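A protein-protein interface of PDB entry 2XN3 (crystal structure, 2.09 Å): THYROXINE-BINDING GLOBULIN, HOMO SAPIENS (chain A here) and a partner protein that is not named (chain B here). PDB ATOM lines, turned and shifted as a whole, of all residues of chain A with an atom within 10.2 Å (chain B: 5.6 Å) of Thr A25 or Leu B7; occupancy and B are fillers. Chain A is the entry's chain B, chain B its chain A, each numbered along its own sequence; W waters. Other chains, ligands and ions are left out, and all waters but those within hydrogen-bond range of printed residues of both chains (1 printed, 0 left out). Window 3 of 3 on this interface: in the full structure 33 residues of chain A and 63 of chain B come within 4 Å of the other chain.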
ATOM      1  N   ILE A  20      -0.013 -32.683  19.654  1.00  0.00           N
ATOM      2  CA  ILE A  20       1.191 -33.296  20.187  1.00  0.00           C
ATOM      3  C   ILE A  20       1.554 -32.559  21.464  1.00  0.00           C
ATOM      4  O   ILE A  20       1.767 -31.335  21.445  1.00  0.00           O
ATOM      5  CB  ILE A  20       2.352 -33.242  19.196  1.00  0.00           C
ATOM      6  CG1 ILE A  20       2.011 -34.076  17.958  1.00  0.00           C
ATOM      7  CG2 ILE A  20       3.635 -33.751  19.870  1.00  0.00           C
ATOM      8  CD1 ILE A  20       2.992 -33.830  16.758  1.00  0.00           C
ATOM      9  N   LEU A  21       1.549 -33.309  22.564  1.00  0.00           N
ATOM     10  CA  LEU A  21       1.606 -32.751  23.908  1.00  0.00           C
ATOM     11  C   LEU A  21       2.870 -33.250  24.591  1.00  0.00           C
ATOM     12  O   LEU A  21       3.240 -34.412  24.439  1.00  0.00           O
ATOM     13  CB  LEU A  21       0.357 -33.168  24.726  1.00  0.00           C
ATOM     14  CG  LEU A  21      -1.030 -32.962  24.045  1.00  0.00           C
ATOM     15  CD1 LEU A  21      -2.153 -33.605  24.839  1.00  0.00           C
ATOM     16  CD2 LEU A  21      -1.350 -31.510  23.843  1.00  0.00           C
ATOM     17  N   GLU A  22       3.537 -32.364  25.333  1.00  0.00           N
ATOM     18  CA  GLU A  22       4.607 -32.774  26.224  1.00  0.00           C
ATOM     19  C   GLU A  22       4.012 -32.918  27.629  1.00  0.00           C
ATOM     20  O   GLU A  22       3.282 -32.044  28.101  1.00  0.00           O
ATOM     21  CB  GLU A  22       5.778 -31.789  26.154  1.00  0.00           C
ATOM     22  CG  GLU A  22       7.049 -32.297  26.839  1.00  0.00           C
ATOM     23  CD  GLU A  22       7.123 -31.951  28.312  1.00  0.00           C
ATOM     24  OE1 GLU A  22       6.356 -31.086  28.780  1.00  0.00           O
ATOM     25  OE2 GLU A  22       7.975 -32.540  29.001  1.00  0.00           O
ATOM     26  N   ARG A  23       4.357 -34.027  28.291  1.00  0.00           N
ATOM     27  CA  ARG A  23       3.662 -34.464  29.507  1.00  0.00           C
ATOM     28  C   ARG A  23       3.958 -33.607  30.728  1.00  0.00           C
ATOM     29  O   ARG A  23       3.043 -33.143  31.396  1.00  0.00           O
ATOM     30  CB  ARG A  23       4.002 -35.928  29.824  1.00  0.00           C
ATOM     31  CG  ARG A  23       3.315 -36.921  28.922  1.00  0.00           C
ATOM     32  CD  ARG A  23       3.434 -38.347  29.459  1.00  0.00           C
ATOM     33  NE  ARG A  23       2.419 -39.213  28.874  1.00  0.00           N
ATOM     34  CZ  ARG A  23       1.124 -39.139  29.173  1.00  0.00           C
ATOM     35  NH1 ARG A  23       0.256 -39.961  28.600  1.00  0.00           N
ATOM     36  NH2 ARG A  23       0.696 -38.233  30.039  1.00  0.00           N
ATOM     37  N   SER A  24       5.238 -33.408  31.026  1.00  0.00           N
ATOM     38  CA  SER A  24       5.620 -32.765  32.297  1.00  0.00           C
ATOM     39  C   SER A  24       5.162 -31.313  32.434  1.00  0.00           C
ATOM     40  O   SER A  24       4.837 -30.884  33.528  1.00  0.00           O
ATOM     41  CB  SER A  24       7.128 -32.878  32.547  1.00  0.00           C
ATOM     42  OG  SER A  24       7.857 -32.032  31.690  1.00  0.00           O
ATOM     43  N   THR A  25       5.158 -30.556  31.343  1.00  0.00           N
ATOM     44  CA  THR A  25       4.709 -29.167  31.374  1.00  0.00           C
ATOM     45  C   THR A  25       3.248 -29.004  30.940  1.00  0.00           C
ATOM     46  O   THR A  25       2.693 -27.904  31.017  1.00  0.00           O
ATOM     47  CB  THR A  25       5.581 -28.287  30.464  1.00  0.00           C
ATOM     48  OG1 THR A  25       5.350 -28.636  29.091  1.00  0.00           O
ATOM     49  CG2 THR A  25       7.067 -28.463  30.798  1.00  0.00           C
ATOM     50  N   ARG A  26       2.645 -30.095  30.484  1.00  0.00           N
ATOM     51  CA  ARG A  26       1.353 -30.091  29.802  1.00  0.00           C
ATOM     52  C   ARG A  26       1.324 -29.029  28.689  1.00  0.00           C
ATOM     53  O   ARG A  26       0.416 -28.208  28.640  1.00  0.00           O
ATOM     54  CB  ARG A  26       0.223 -29.907  30.831  1.00  0.00           C
ATOM     55  CG  ARG A  26      -0.009 -31.174  31.703  1.00  0.00           C
ATOM     56  CD  ARG A  26      -0.640 -30.866  33.065  1.00  0.00           C
ATOM     57  NE  ARG A  26      -0.551 -32.013  33.977  1.00  0.00           N
ATOM     58  CZ  ARG A  26      -0.819 -31.979  35.284  1.00  0.00           C
ATOM     59  NH1 ARG A  26      -1.205 -30.852  35.879  1.00  0.00           N
ATOM     60  NH2 ARG A  26      -0.700 -33.086  36.006  1.00  0.00           N
ATOM     61  N   SER A  27       2.337 -29.033  27.818  1.00  0.00           N
ATOM     62  CA  SER A  27       2.399 -28.080  26.699  1.00  0.00           C
ATOM     63  C   SER A  27       1.813 -28.701  25.427  1.00  0.00           C
ATOM     64  O   SER A  27       1.993 -29.884  25.168  1.00  0.00           O
ATOM     65  CB  SER A  27       3.846 -27.645  26.401  1.00  0.00           C
ATOM     66  OG  SER A  27       4.377 -26.797  27.393  1.00  0.00           O
ATOM     67  N   ILE A  28       1.139 -27.893  24.625  1.00  0.00           N
ATOM     68  CA  ILE A  28       0.776 -28.300  23.289  1.00  0.00           C
ATOM     69  C   ILE A  28       1.904 -27.872  22.395  1.00  0.00           C
ATOM     70  O   ILE A  28       2.052 -26.670  22.081  1.00  0.00           O
ATOM     71  CB  ILE A  28      -0.533 -27.678  22.803  1.00  0.00           C
ATOM     72  CG1 ILE A  28      -1.674 -27.961  23.788  1.00  0.00           C
ATOM     73  CG2 ILE A  28      -0.877 -28.243  21.435  1.00  0.00           C
ATOM     74  CD1 ILE A  28      -3.001 -27.365  23.340  1.00  0.00           C
ATOM     75  N   LEU A  29       2.720 -28.845  22.005  1.00  0.00           N
ATOM     76  CA  LEU A  29       3.842 -28.593  21.115  1.00  0.00           C
ATOM     77  C   LEU A  29       3.360 -28.276  19.694  1.00  0.00           C
ATOM     78  O   LEU A  29       3.870 -27.356  19.046  1.00  0.00           O
ATOM     79  CB  LEU A  29       4.802 -29.791  21.096  1.00  0.00           C
ATOM     80  CG  LEU A  29       5.372 -30.229  22.449  1.00  0.00           C
ATOM     81  CD1 LEU A  29       6.315 -31.440  22.267  1.00  0.00           C
ATOM     82  CD2 LEU A  29       6.094 -29.088  23.204  1.00  0.00           C
ATOM     83  N   LEU B   7       3.294 -24.222  36.807  1.00  0.00           N
ATOM     84  CA  LEU B   7       3.411 -24.277  35.318  1.00  0.00           C
ATOM     85  C   LEU B   7       2.080 -24.584  34.610  1.00  0.00           C
ATOM     86  O   LEU B   7       1.841 -24.110  33.501  1.00  0.00           O
ATOM     87  CB  LEU B   7       4.464 -25.321  34.890  1.00  0.00           C
ATOM     88  CG  LEU B   7       5.883 -24.864  34.506  1.00  0.00           C
ATOM     89  CD1 LEU B   7       6.637 -26.004  33.785  1.00  0.00           C
ATOM     90  CD2 LEU B   7       5.892 -23.598  33.639  1.00  0.00           C
ATOM     91  N   TYR B   8       1.221 -25.371  35.243  1.00  0.00           N
ATOM     92  CA  TYR B   8       0.041 -25.912  34.555  1.00  0.00           C
ATOM     93  C   TYR B   8      -1.025 -24.851  34.281  1.00  0.00           C
ATOM     94  O   TYR B   8      -1.732 -24.927  33.270  1.00  0.00           O
ATOM     95  CB  TYR B   8      -0.540 -27.109  35.330  1.00  0.00           C
ATOM     96  CG  TYR B   8       0.522 -28.129  35.707  1.00  0.00           C
ATOM     97  CD1 TYR B   8       1.452 -28.571  34.763  1.00  0.00           C
ATOM     98  CD2 TYR B   8       0.615 -28.630  37.008  1.00  0.00           C
ATOM     99  CE1 TYR B   8       2.433 -29.487  35.092  1.00  0.00           C
ATOM    100  CE2 TYR B   8       1.604 -29.559  37.357  1.00  0.00           C
ATOM    101  CZ  TYR B   8       2.508 -29.983  36.390  1.00  0.00           C
ATOM    102  OH  TYR B   8       3.491 -30.900  36.706  1.00  0.00           O
ATOM    103  N   LYS B   9      -1.127 -23.864  35.170  1.00  0.00           N
ATOM    104  CA  LYS B   9      -2.045 -22.746  34.968  1.00  0.00           C
ATOM    105  C   LYS B   9      -1.565 -21.860  33.811  1.00  0.00           C
ATOM    106  O   LYS B   9      -2.375 -21.248  33.110  1.00  0.00           O
ATOM    107  CB  LYS B   9      -2.208 -21.950  36.257  1.00  0.00           C
ATOM    108  CG  LYS B   9      -2.627 -22.832  37.434  1.00  0.00           C
ATOM    109  CD  LYS B   9      -3.536 -22.105  38.406  1.00  0.00           C
ATOM    110  CE  LYS B   9      -3.870 -22.981  39.588  1.00  0.00           C
ATOM    111  NZ  LYS B   9      -4.348 -22.164  40.732  1.00  0.00           N
ATOM    112  N   MET B  10      -0.252 -21.820  33.604  1.00  0.00           N
ATOM    113  CA  MET B  10       0.323 -21.175  32.428  1.00  0.00           C
ATOM    114  C   MET B  10       0.020 -21.998  31.184  1.00  0.00           C
ATOM    115  O   MET B  10      -0.456 -21.470  30.175  1.00  0.00           O
ATOM    116  CB  MET B  10       1.838 -21.020  32.582  1.00  0.00           C
ATOM    117  CG  MET B  10       2.590 -20.709  31.287  1.00  0.00           C
ATOM    118  SD  MET B  10       4.226 -19.978  31.586  1.00  0.00           S
ATOM    119  CE  MET B  10       3.757 -18.450  32.407  1.00  0.00           C
ATOM    120  N   SER B  11       0.313 -23.295  31.249  1.00  0.00           N
ATOM    121  CA  SER B  11       0.106 -24.167  30.093  1.00  0.00           C
ATOM    122  C   SER B  11      -1.371 -24.338  29.750  1.00  0.00           C
ATOM    123  O   SER B  11      -1.712 -24.565  28.600  1.00  0.00           O
ATOM    124  CB  SER B  11       0.808 -25.509  30.285  1.00  0.00           C
ATOM    125  OG  SER B  11       2.209 -25.328  30.122  1.00  0.00           O
ATOM    126  N   SER B  12      -2.242 -24.166  30.730  1.00  0.00           N
ATOM    127  CA  SER B  12      -3.666 -24.094  30.459  1.00  0.00           C
ATOM    128  C   SER B  12      -4.087 -22.821  29.699  1.00  0.00           C
ATOM    129  O   SER B  12      -4.925 -22.874  28.796  1.00  0.00           O
ATOM    130  CB  SER B  12      -4.450 -24.190  31.742  1.00  0.00           C
ATOM    131  OG  SER B  12      -5.822 -24.258  31.442  1.00  0.00           O
ATOM    132  N   GLY B  79       7.646 -17.778  34.461  1.00  0.00           N
ATOM    133  CA  GLY B  79       6.998 -19.013  33.999  1.00  0.00           C
ATOM    134  C   GLY B  79       7.471 -19.491  32.628  1.00  0.00           C
ATOM    135  O   GLY B  79       7.724 -20.685  32.436  1.00  0.00           O
ATOM    136  N   HIS B  82      11.046 -20.836  32.805  1.00  0.00           N
ATOM    137  CA  HIS B  82      11.021 -22.210  33.339  1.00  0.00           C
ATOM    138  C   HIS B  82      10.415 -23.215  32.316  1.00  0.00           C
ATOM    139  O   HIS B  82      10.899 -24.338  32.183  1.00  0.00           O
ATOM    140  CB  HIS B  82      10.265 -22.232  34.676  1.00  0.00           C
ATOM    141  CG  HIS B  82      10.180 -23.588  35.315  1.00  0.00           C
ATOM    142  ND1 HIS B  82       9.113 -23.972  36.103  1.00  0.00           N
ATOM    143  CD2 HIS B  82      11.015 -24.655  35.272  1.00  0.00           C
ATOM    144  CE1 HIS B  82       9.300 -25.211  36.525  1.00  0.00           C
ATOM    145  NE2 HIS B  82      10.446 -25.648  36.034  1.00  0.00           N
ATOM    146  N   LEU B  83       9.383 -22.801  31.581  1.00  0.00           N
ATOM    147  CA  LEU B  83       8.820 -23.637  30.506  1.00  0.00           C
ATOM    148  C   LEU B  83       9.866 -24.020  29.441  1.00  0.00           C
ATOM    149  O   LEU B  83      10.023 -25.205  29.127  1.00  0.00           O
ATOM    150  CB  LEU B  83       7.618 -22.942  29.837  1.00  0.00           C
ATOM    151  CG  LEU B  83       6.794 -23.740  28.804  1.00  0.00           C
ATOM    152  CD1 LEU B  83       6.096 -24.930  29.448  1.00  0.00           C
ATOM    153  CD2 LEU B  83       5.766 -22.856  28.089  1.00  0.00           C
ATOM    154  N   SER B  86      12.518 -26.311  30.803  1.00  0.00           N
ATOM    155  CA  SER B  86      12.002 -27.654  31.010  1.00  0.00           C
ATOM    156  C   SER B  86      11.873 -28.455  29.688  1.00  0.00           C
ATOM    157  O   SER B  86      12.338 -29.588  29.605  1.00  0.00           O
ATOM    158  CB  SER B  86      10.661 -27.563  31.721  1.00  0.00           C
ATOM    159  OG  SER B  86      10.258 -28.832  32.145  1.00  0.00           O
ATOM    160  N   LEU B  87      11.297 -27.848  28.651  1.00  0.00           N
ATOM    161  CA  LEU B  87      11.134 -28.531  27.358  1.00  0.00           C
ATOM    162  C   LEU B  87      12.497 -28.950  26.783  1.00  0.00           C
ATOM    163  O   LEU B  87      12.635 -30.034  26.220  1.00  0.00           O
ATOM    164  CB  LEU B  87      10.359 -27.657  26.368  1.00  0.00           C
ATOM    165  CG  LEU B  87       8.896 -27.342  26.730  1.00  0.00           C
ATOM    166  CD1 LEU B  87       8.324 -26.313  25.787  1.00  0.00           C
ATOM    167  CD2 LEU B  87       8.009 -28.587  26.717  1.00  0.00           C
HETATM  168  O   HOH W   1       2.805 -24.388  27.053  1.00  0.00           O
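OG1 of Thr A25 lies within hydrogen-bond range of OE1 of Glu A22.
The backbone NH (N) of Glu A22 lies within hydrogen-bond range of the backbone carbonyl oxygen (O) of Ser A27, at 2.9 Å.
OG of Ser A24 sits at hydrogen-bond distance from OE2 of Glu A22.
OG1 of Thr A25 is in hydrogen-bond range of OG of Ser A27 (2.7 Å).
Of the printed residues of chain B, Thr A25 touches Leu B7 (3.9 Å), Ser B11 (2.8 Å), Leu B83 (3.5 Å), Ser B86 (3.5 Å) and Leu B87 (3.6 Å).
Leu B7 touches one residue of chain A.
Met B10 touches none of the printed residues of chain A.
Ser B11 touches three residues of chain A.
No residue of chain A comes within 4 Å of Gly B79.
His B82 touches none of the printed residues of chain A.
Of the printed residues of chain A, Ser B86 touches Thr A25.
Printed residues of chain B within 4 Å of Glu A22: Leu B87 (3.6 Å).
Of the printed residues of chain B, Ser A27 touches Ser B11 and Leu B83.
Printed residues of chain B within 4 Å of Ser A24: Tyr B8 (3.2 Å).
Of the printed residues of chain B, Arg A26 touches Tyr B8 (3.1 Å) and Ser B11 (3.2 Å).
The nearest printed residue of chain B that does not touch Thr A25 is Tyr B8 (4.002 Å).
The nearest residue of chain A that does not touch Leu B7 is Ser A24 (5.2 Å).
The nearest printed residue of chain A that does not touch Tyr B8 is Thr A25 (4.002 Å).
O of Thr A25 sits at hydrogen-bond distance from OG of Ser B11 (2.8 Å).
The backbone carbonyl oxygen (O) of Ser A24 lies close to the side-chain hydroxyl (OH) of Tyr B8 (3.5 Å).
Among the printed residues, no Asp or Glu carboxylate lies within 4 Å of a Lys or Arg side-chain nitrogen of the other chain.
OE1 of Glu A22 touches CD2 of Leu B87 (3.6 Å).
Leu B7 touches Thr A25.
Leu B83 touches Thr A25.
Ser B86 touches Thr A25.
Thr A25 touches Leu B87.
Arg A26 touches Tyr B8.
Arg A26 touches Ser B11 (O to CB, 3.2 Å).
Ser B11 touches Ser A27 (OG to OG, 3.8 Å).
Ser A27 touches Leu B83 (OG to CD1, 3.3 Å).
Water W1 lies within hydrogen-bond range of the side-chain hydroxyl of Ser A27 (2.9 Å) and the side-chain hydroxyl of Ser B11 (3.3 Å).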
